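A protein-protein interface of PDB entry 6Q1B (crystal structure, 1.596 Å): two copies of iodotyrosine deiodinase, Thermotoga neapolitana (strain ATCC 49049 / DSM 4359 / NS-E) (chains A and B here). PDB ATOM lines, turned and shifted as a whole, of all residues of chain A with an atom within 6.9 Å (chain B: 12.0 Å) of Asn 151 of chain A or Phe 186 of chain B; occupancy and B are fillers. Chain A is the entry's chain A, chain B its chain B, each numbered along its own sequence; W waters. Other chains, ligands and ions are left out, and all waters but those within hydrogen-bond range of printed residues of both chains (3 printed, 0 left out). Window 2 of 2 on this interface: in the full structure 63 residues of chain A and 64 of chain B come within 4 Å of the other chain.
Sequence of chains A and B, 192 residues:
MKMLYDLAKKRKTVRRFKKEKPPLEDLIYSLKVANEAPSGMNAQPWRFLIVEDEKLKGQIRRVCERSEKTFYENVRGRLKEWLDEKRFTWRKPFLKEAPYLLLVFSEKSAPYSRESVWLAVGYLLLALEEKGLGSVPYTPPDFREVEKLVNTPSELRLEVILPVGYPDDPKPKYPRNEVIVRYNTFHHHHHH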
ATOM      1  N   ARG A  47     -14.547   7.259  -4.793  1.00  0.00           N
ATOM      2  CA  ARG A  47     -14.740   8.690  -4.901  1.00  0.00           C
ATOM      3  C   ARG A  47     -13.731   9.157  -5.890  1.00  0.00           C
ATOM      4  O   ARG A  47     -12.597   8.654  -5.916  1.00  0.00           O
ATOM      5  CB  ARG A  47     -14.531   9.409  -3.589  1.00  0.00           C
ATOM      6  CG  ARG A  47     -15.415   8.954  -2.470  1.00  0.00           C
ATOM      7  CD  ARG A  47     -16.830   9.385  -2.697  1.00  0.00           C
ATOM      8  NE  ARG A  47     -17.586   9.030  -1.518  1.00  0.00           N
ATOM      9  CZ  ARG A  47     -18.075   7.816  -1.270  1.00  0.00           C
ATOM     10  NH1 ARG A  47     -17.932   6.842  -2.161  1.00  0.00           N
ATOM     11  NH2 ARG A  47     -18.720   7.589  -0.131  1.00  0.00           N
ATOM     12  N   PHE A  48     -14.141  10.107  -6.705  1.00  0.00           N
ATOM     13  CA  PHE A  48     -13.310  10.597  -7.776  1.00  0.00           C
ATOM     14  C   PHE A  48     -12.981  12.049  -7.621  1.00  0.00           C
ATOM     15  O   PHE A  48     -13.857  12.900  -7.391  1.00  0.00           O
ATOM     16  CB  PHE A  48     -14.008  10.360  -9.094  1.00  0.00           C
ATOM     17  CG  PHE A  48     -14.341   8.931  -9.326  1.00  0.00           C
ATOM     18  CD1 PHE A  48     -13.340   7.995  -9.517  1.00  0.00           C
ATOM     19  CD2 PHE A  48     -15.653   8.514  -9.353  1.00  0.00           C
ATOM     20  CE1 PHE A  48     -13.659   6.670  -9.736  1.00  0.00           C
ATOM     21  CE2 PHE A  48     -15.959   7.181  -9.578  1.00  0.00           C
ATOM     22  CZ  PHE A  48     -14.968   6.284  -9.756  1.00  0.00           C
ATOM     23  N   LEU A  49     -11.696  12.332  -7.796  1.00  0.00           N
ATOM     24  CA  LEU A  49     -11.208  13.671  -7.795  1.00  0.00           C
ATOM     25  C   LEU A  49     -10.513  13.886  -9.100  1.00  0.00           C
ATOM     26  O   LEU A  49      -9.579  13.199  -9.425  1.00  0.00           O
ATOM     27  CB  LEU A  49     -10.277  13.898  -6.624  1.00  0.00           C
ATOM     28  CG  LEU A  49      -9.640  15.279  -6.548  1.00  0.00           C
ATOM     29  CD1 LEU A  49     -10.691  16.317  -6.161  1.00  0.00           C
ATOM     30  CD2 LEU A  49      -8.525  15.276  -5.538  1.00  0.00           C
ATOM     31  N   LEU A 103      -7.967  11.074  -9.590  1.00  0.00           N
ATOM     32  CA  LEU A 103      -7.592  10.474  -8.340  1.00  0.00           C
ATOM     33  C   LEU A 103      -8.772   9.702  -7.842  1.00  0.00           C
ATOM     34  O   LEU A 103      -9.875  10.211  -7.739  1.00  0.00           O
ATOM     35  CB  LEU A 103      -7.132  11.515  -7.334  1.00  0.00           C
ATOM     36  CG  LEU A 103      -5.656  11.877  -7.432  1.00  0.00           C
ATOM     37  CD1 LEU A 103      -5.328  12.411  -8.830  1.00  0.00           C
ATOM     38  CD2 LEU A 103      -5.330  12.914  -6.388  1.00  0.00           C
ATOM     39  N   PHE A 105     -10.365   7.398  -4.970  1.00  0.00           N
ATOM     40  CA  PHE A 105     -10.277   7.140  -3.564  1.00  0.00           C
ATOM     41  C   PHE A 105     -11.225   6.048  -3.162  1.00  0.00           C
ATOM     42  O   PHE A 105     -12.214   5.836  -3.827  1.00  0.00           O
ATOM     43  CB  PHE A 105     -10.642   8.374  -2.765  1.00  0.00           C
ATOM     44  CG  PHE A 105      -9.759   9.529  -2.997  1.00  0.00           C
ATOM     45  CD1 PHE A 105      -9.921  10.317  -4.127  1.00  0.00           C
ATOM     46  CD2 PHE A 105      -8.771   9.854  -2.092  1.00  0.00           C
ATOM     47  CE1 PHE A 105      -9.102  11.415  -4.337  1.00  0.00           C
ATOM     48  CE2 PHE A 105      -7.943  10.948  -2.322  1.00  0.00           C
ATOM     49  CZ  PHE A 105      -8.119  11.707  -3.449  1.00  0.00           C
ATOM     50  N   VAL A 146       0.363  13.121  -1.415  1.00  0.00           N
ATOM     51  CA  VAL A 146      -0.566  13.453  -2.476  1.00  0.00           C
ATOM     52  C   VAL A 146      -1.928  13.672  -1.868  1.00  0.00           C
ATOM     53  O   VAL A 146      -2.612  14.619  -2.229  1.00  0.00           O
ATOM     54  CB  VAL A 146      -0.632  12.381  -3.550  1.00  0.00           C
ATOM     55  CG1 VAL A 146      -1.670  12.713  -4.578  1.00  0.00           C
ATOM     56  CG2 VAL A 146       0.707  12.303  -4.219  1.00  0.00           C
ATOM     57  N   GLU A 147      -2.301  12.801  -0.935  1.00  0.00           N
ATOM     58  CA  GLU A 147      -3.584  12.970  -0.271  1.00  0.00           C
ATOM     59  C   GLU A 147      -3.659  14.342   0.347  1.00  0.00           C
ATOM     60  O   GLU A 147      -4.696  15.009   0.256  1.00  0.00           O
ATOM     61  CB  GLU A 147      -3.784  11.930   0.808  1.00  0.00           C
ATOM     62  CG  GLU A 147      -4.133  10.575   0.270  1.00  0.00           C
ATOM     63  CD  GLU A 147      -4.500   9.630   1.384  1.00  0.00           C
ATOM     64  OE1 GLU A 147      -4.430  10.054   2.557  1.00  0.00           O
ATOM     65  OE2 GLU A 147      -4.876   8.480   1.105  1.00  0.00           O
ATOM     66  N   LYS A 148      -2.590  14.753   1.008  1.00  0.00           N
ATOM     67  CA  LYS A 148      -2.615  16.030   1.682  1.00  0.00           C
ATOM     68  C   LYS A 148      -2.746  17.180   0.681  1.00  0.00           C
ATOM     69  O   LYS A 148      -3.433  18.166   0.939  1.00  0.00           O
ATOM     70  CB  LYS A 148      -1.365  16.179   2.547  1.00  0.00           C
ATOM     71  CG  LYS A 148      -1.385  17.392   3.456  1.00  0.00           C
ATOM     72  CD  LYS A 148      -0.269  17.338   4.485  1.00  0.00           C
ATOM     73  CE  LYS A 148      -0.510  18.349   5.599  1.00  0.00           C
ATOM     74  NZ  LYS A 148      -0.806  19.705   5.053  1.00  0.00           N
ATOM     75  N   LEU A 149      -2.082  17.057  -0.470  1.00  0.00           N
ATOM     76  CA  LEU A 149      -2.127  18.102  -1.484  1.00  0.00           C
ATOM     77  C   LEU A 149      -3.523  18.447  -1.945  1.00  0.00           C
ATOM     78  O   LEU A 149      -3.818  19.600  -2.289  1.00  0.00           O
ATOM     79  CB  LEU A 149      -1.326  17.698  -2.711  1.00  0.00           C
ATOM     80  CG  LEU A 149       0.162  17.933  -2.619  1.00  0.00           C
ATOM     81  CD1 LEU A 149       0.782  17.377  -3.890  1.00  0.00           C
ATOM     82  CD2 LEU A 149       0.452  19.414  -2.464  1.00  0.00           C
ATOM     83  N   VAL A 150      -4.380  17.449  -1.944  1.00  0.00           N
ATOM     84  CA  VAL A 150      -5.738  17.652  -2.405  1.00  0.00           C
ATOM     85  C   VAL A 150      -6.723  17.655  -1.229  1.00  0.00           C
ATOM     86  O   VAL A 150      -7.925  17.549  -1.428  1.00  0.00           O
ATOM     87  CB  VAL A 150      -6.115  16.598  -3.446  1.00  0.00           C
ATOM     88  CG1 VAL A 150      -5.180  16.704  -4.659  1.00  0.00           C
ATOM     89  CG2 VAL A 150      -6.070  15.194  -2.879  1.00  0.00           C
ATOM     90  N   ASN A 151      -6.208  17.761  -0.015  1.00  0.00           N
ATOM     91  CA  ASN A 151      -7.052  17.905   1.163  1.00  0.00           C
ATOM     92  C   ASN A 151      -7.960  16.698   1.330  1.00  0.00           C
ATOM     93  O   ASN A 151      -9.154  16.827   1.635  1.00  0.00           O
ATOM     94  CB  ASN A 151      -7.878  19.178   1.063  1.00  0.00           C
ATOM     95  CG  ASN A 151      -8.491  19.570   2.384  1.00  0.00           C
ATOM     96  OD1 ASN A 151      -7.840  19.501   3.430  1.00  0.00           O
ATOM     97  ND2 ASN A 151      -9.762  19.962   2.352  1.00  0.00           N
ATOM     98  N   THR A 152      -7.391  15.523   1.120  1.00  0.00           N
ATOM     99  CA  THR A 152      -8.155  14.304   1.239  1.00  0.00           C
ATOM    100  C   THR A 152      -8.733  14.191   2.615  1.00  0.00           C
ATOM    101  O   THR A 152      -8.014  14.321   3.600  1.00  0.00           O
ATOM    102  CB  THR A 152      -7.300  13.086   0.990  1.00  0.00           C
ATOM    103  OG1 THR A 152      -6.713  13.207  -0.303  1.00  0.00           O
ATOM    104  CG2 THR A 152      -8.119  11.842   1.033  1.00  0.00           C
ATOM    105  N   PRO A 153     -10.031  13.940   2.688  1.00  0.00           N
ATOM    106  CA  PRO A 153     -10.626  13.709   4.000  1.00  0.00           C
ATOM    107  C   PRO A 153     -10.110  12.435   4.594  1.00  0.00           C
ATOM    108  O   PRO A 153      -9.800  11.510   3.877  1.00  0.00           O
ATOM    109  CB  PRO A 153     -12.117  13.601   3.707  1.00  0.00           C
ATOM    110  CG  PRO A 153     -12.271  13.599   2.289  1.00  0.00           C
ATOM    111  CD  PRO A 153     -11.044  14.054   1.630  1.00  0.00           C
ATOM    112  N   SER A 154     -10.031  12.374   5.909  1.00  0.00           N
ATOM    113  CA  SER A 154      -9.480  11.203   6.558  1.00  0.00           C
ATOM    114  C   SER A 154     -10.254   9.934   6.207  1.00  0.00           C
ATOM    115  O   SER A 154      -9.743   8.831   6.349  1.00  0.00           O
ATOM    116  CB  SER A 154      -9.485  11.396   8.062  1.00  0.00           C
ATOM    117  OG  SER A 154     -10.796  11.713   8.484  1.00  0.00           O
ATOM    118  N   LEU A 156     -11.160   8.870   3.400  1.00  0.00           N
ATOM    119  CA  LEU A 156     -10.884   8.388   2.073  1.00  0.00           C
ATOM    120  C   LEU A 156      -9.429   8.046   1.937  1.00  0.00           C
ATOM    121  O   LEU A 156      -8.566   8.698   2.494  1.00  0.00           O
ATOM    122  CB  LEU A 156     -11.262   9.419   1.024  1.00  0.00           C
ATOM    123  CG  LEU A 156     -12.722   9.862   1.011  1.00  0.00           C
ATOM    124  CD1 LEU A 156     -12.950  10.852  -0.108  1.00  0.00           C
ATOM    125  CD2 LEU A 156     -13.628   8.680   0.828  1.00  0.00           C
ATOM    126  N   VAL B 179     -22.444   9.329  -9.776  1.00  0.00           N
ATOM    127  CA  VAL B 179     -21.126   9.795  -9.405  1.00  0.00           C
ATOM    128  C   VAL B 179     -21.207  11.282  -9.163  1.00  0.00           C
ATOM    129  O   VAL B 179     -21.781  12.033  -9.962  1.00  0.00           O
ATOM    130  CB  VAL B 179     -20.097   9.521 -10.486  1.00  0.00           C
ATOM    131  CG1 VAL B 179     -18.743  10.091 -10.081  1.00  0.00           C
ATOM    132  CG2 VAL B 179     -20.008   8.039 -10.724  1.00  0.00           C
ATOM    133  N   ILE B 180     -20.634  11.697  -8.050  1.00  0.00           N
ATOM    134  CA  ILE B 180     -20.446  13.095  -7.768  1.00  0.00           C
ATOM    135  C   ILE B 180     -18.956  13.299  -7.723  1.00  0.00           C
ATOM    136  O   ILE B 180     -18.268  12.831  -6.816  1.00  0.00           O
ATOM    137  CB  ILE B 180     -21.098  13.516  -6.471  1.00  0.00           C
ATOM    138  CG1 ILE B 180     -22.605  13.221  -6.555  1.00  0.00           C
ATOM    139  CG2 ILE B 180     -20.844  14.989  -6.235  1.00  0.00           C
ATOM    140  CD1 ILE B 180     -23.327  13.338  -5.251  1.00  0.00           C
ATOM    141  N   VAL B 181     -18.462  13.969  -8.744  1.00  0.00           N
ATOM    142  CA  VAL B 181     -17.038  14.213  -8.850  1.00  0.00           C
ATOM    143  C   VAL B 181     -16.682  15.431  -8.053  1.00  0.00           C
ATOM    144  O   VAL B 181     -17.509  16.269  -7.731  1.00  0.00           O
ATOM    145  CB  VAL B 181     -16.590  14.421 -10.294  1.00  0.00           C
ATOM    146  CG1 VAL B 181     -16.859  13.171 -11.098  1.00  0.00           C
ATOM    147  CG2 VAL B 181     -17.279  15.626 -10.911  1.00  0.00           C
ATOM    148  N   ARG B 182     -15.415  15.469  -7.702  1.00  0.00           N
ATOM    149  CA  ARG B 182     -14.794  16.646  -7.192  1.00  0.00           C
ATOM    150  C   ARG B 182     -13.692  17.006  -8.133  1.00  0.00           C
ATOM    151  O   ARG B 182     -13.222  16.165  -8.897  1.00  0.00           O
ATOM    152  CB  ARG B 182     -14.272  16.385  -5.804  1.00  0.00           C
ATOM    153  CG  ARG B 182     -15.383  16.162  -4.816  1.00  0.00           C
ATOM    154  CD  ARG B 182     -14.766  15.741  -3.550  1.00  0.00           C
ATOM    155  NE  ARG B 182     -15.677  15.835  -2.422  1.00  0.00           N
ATOM    156  CZ  ARG B 182     -16.450  14.839  -2.003  1.00  0.00           C
ATOM    157  NH1 ARG B 182     -16.456  13.668  -2.638  1.00  0.00           N
ATOM    158  NH2 ARG B 182     -17.225  15.024  -0.948  1.00  0.00           N
ATOM    159  N   TYR B 183     -13.328  18.270  -8.087  1.00  0.00           N
ATOM    160  CA  TYR B 183     -12.281  18.812  -8.918  1.00  0.00           C
ATOM    161  C   TYR B 183     -11.156  19.363  -8.100  1.00  0.00           C
ATOM    162  O   TYR B 183     -11.361  20.143  -7.170  1.00  0.00           O
ATOM    163  CB  TYR B 183     -12.835  19.901  -9.798  1.00  0.00           C
ATOM    164  CG  TYR B 183     -13.879  19.400 -10.742  1.00  0.00           C
ATOM    165  CD1 TYR B 183     -15.197  19.318 -10.355  1.00  0.00           C
ATOM    166  CD2 TYR B 183     -13.535  18.980 -12.016  1.00  0.00           C
ATOM    167  CE1 TYR B 183     -16.154  18.856 -11.209  1.00  0.00           C
ATOM    168  CE2 TYR B 183     -14.486  18.506 -12.880  1.00  0.00           C
ATOM    169  CZ  TYR B 183     -15.797  18.450 -12.466  1.00  0.00           C
ATOM    170  OH  TYR B 183     -16.780  17.984 -13.297  1.00  0.00           O
ATOM    171  N   ASN B 184      -9.971  18.929  -8.497  1.00  0.00           N
ATOM    172  CA  ASN B 184      -8.688  19.389  -8.010  1.00  0.00           C
ATOM    173  C   ASN B 184      -8.421  19.100  -6.562  1.00  0.00           C
ATOM    174  O   ASN B 184      -7.482  18.388  -6.252  1.00  0.00           O
ATOM    175  CB  ASN B 184      -8.549  20.866  -8.293  1.00  0.00           C
ATOM    176  CG  ASN B 184      -8.407  21.115  -9.761  1.00  0.00           C
ATOM    177  OD1 ASN B 184      -7.617  20.442 -10.422  1.00  0.00           O
ATOM    178  ND2 ASN B 184      -9.182  22.041 -10.296  1.00  0.00           N
ATOM    179  N   THR B 185      -9.243  19.636  -5.674  1.00  0.00           N
ATOM    180  CA  THR B 185      -9.098  19.305  -4.276  1.00  0.00           C
ATOM    181  C   THR B 185     -10.451  19.132  -3.649  1.00  0.00           C
ATOM    182  O   THR B 185     -11.473  19.563  -4.186  1.00  0.00           O
ATOM    183  CB  THR B 185      -8.340  20.376  -3.497  1.00  0.00           C
ATOM    184  OG1 THR B 185      -9.138  21.547  -3.434  1.00  0.00           O
ATOM    185  CG2 THR B 185      -7.023  20.717  -4.182  1.00  0.00           C
ATOM    186  N   PHE B 186     -10.433  18.484  -2.497  1.00  0.00           N
ATOM    187  CA  PHE B 186     -11.604  18.435  -1.630  1.00  0.00           C
ATOM    188  C   PHE B 186     -11.764  19.793  -0.954  1.00  0.00           C
ATOM    189  O   PHE B 186     -10.762  20.378  -0.547  1.00  0.00           O
ATOM    190  CB  PHE B 186     -11.434  17.341  -0.589  1.00  0.00           C
ATOM    191  CG  PHE B 186     -11.414  15.963  -1.154  1.00  0.00           C
ATOM    192  CD1 PHE B 186     -10.236  15.405  -1.624  1.00  0.00           C
ATOM    193  CD2 PHE B 186     -12.572  15.206  -1.182  1.00  0.00           C
ATOM    194  CE1 PHE B 186     -10.223  14.137  -2.135  1.00  0.00           C
ATOM    195  CE2 PHE B 186     -12.578  13.938  -1.688  1.00  0.00           C
ATOM    196  CZ  PHE B 186     -11.388  13.386  -2.165  1.00  0.00           C
HETATM  197  O   HOH W   1     -15.614  12.865  -5.112  1.00  0.00           O
HETATM  198  O   HOH W   2     -16.899  10.860  -6.899  1.00  0.00           O
HETATM  199  O   HOH W   3     -17.140  11.704  -0.072  1.00  0.00           O
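O of Phe 48 of chain A is in hydrogen-bond range of N of Arg 182 of chain B (3.0 Å).
The backbone carbonyl oxygen (O) of Val 150 of chain A lies within hydrogen-bond range of the backbone NH (N) of Phe 186 of chain B, 2.9 Å away.
The side-chain amide nitrogen (ND2) of Asn 151 of chain A lies within hydrogen-bond range of the backbone carbonyl oxygen (O) of Phe 186 of chain B (3.1 Å).
O of Arg 47 of chain A sits at hydrogen-bond distance from N of Phe 105 of chain A, at 2.7 Å.
The backbone carbonyl oxygen (O) of Leu 49 of chain A lies within hydrogen-bond range of the backbone NH (N) of Leu 103 of chain A (2.7 Å).
O of Glu 147 of chain A is in hydrogen-bond range of OG1 of Thr 152 of chain A (2.8 Å).
Among the printed residues, merely in contact across the chains: Phe 48 of chain A with Val 179 of chain B, Phe 48 of chain A with Val 181 of chain B, Leu 49 of chain A with Arg 182 of chain B, Leu 49 of chain A with Tyr 183 of chain B, Leu 49 of chain A with Asn 184 of chain B, Leu 49 of chain A with Thr 185 of chain B, Leu 49 of chain A with Phe 186 of chain B, Phe 105 of chain A with Phe 186 of chain B, Leu 149 of chain A with Thr 185 of chain B, Val 150 of chain A with Asn 184 of chain B, Val 150 of chain A with Thr 185 of chain B, Thr 152 of chain A with Phe 186 of chain B, Pro 153 of chain A with Phe 186 of chain B and Leu 156 of chain A with Phe 186 of chain B.
Of the printed residues of chain B, Asn 151 of chain A touches Phe 186.
Of the printed residues of chain A, Phe 186 of chain B touches Leu 49, Phe 105, Val 150, Asn 151, Thr 152, Pro 153 and Leu 156.
Leu 49 of chain A touches just these residues of chain B: Arg 182 (3.4 Å), Tyr 183 (3.6 Å), Asn 184 (3.4 Å), Thr 185 (3.7 Å) and Phe 186 (3.97 Å).
Printed residues of chain B within 4 Å of Phe 105 of chain A: Phe 186 (3.5 Å).
No residue of chain B comes within 4 Å of Lys 148 of chain A.
Of chain B, only Phe 186 comes within 4 Å of Thr 152 of chain A.
Pro 153 of chain A touches just one residue of chain B: Phe 186.
Printed residues of chain B within 4 Å of Leu 149 of chain A: Thr 185 (3.9 Å).
Of the printed residues of chain A, Tyr 183 of chain B touches Leu 49.
Ser 154 of chain A touches none of the printed residues of chain B.
Leu 103 of chain A touches none of the printed residues of chain B.
The nearest printed residue of chain B that does not touch Asn 151 of chain A is Thr 185 of chain B (4.7 Å).
Of the 15 printed residues of chain A, 9 touch a printed residue of chain B.
Printed residues of chain A that touch a printed residue of chain B: Phe 48, Leu 49, Phe 105, Leu 149, Val 150, Asn 151, Thr 152, Pro 153 and Leu 156.
Among the printed residues, 17 pairs touch across the chains.
Among the printed residues, no Asp or Glu carboxylate lies within 4 Å of a Lys or Arg side-chain nitrogen of the other chain.
No position is printed for both chains.
Of the 17 pairs that touch across the chains among the printed residues, none has its exchanged pair printed and touching as well.
Water W2 bridges O of Ile 180 of chain B and N of Phe 48 of chain A.
Water W1 lies within hydrogen-bond range of NH1 of Arg 182 of chain B (2.7 Å), O of Phe 48 of chain A (2.9 Å) and O of Ile 180 of chain B (3.2 Å).
Water W3 lies within hydrogen-bond range of the guanidinium group of Arg 47 of chain A and the guanidinium group of Arg 182 of chain B.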
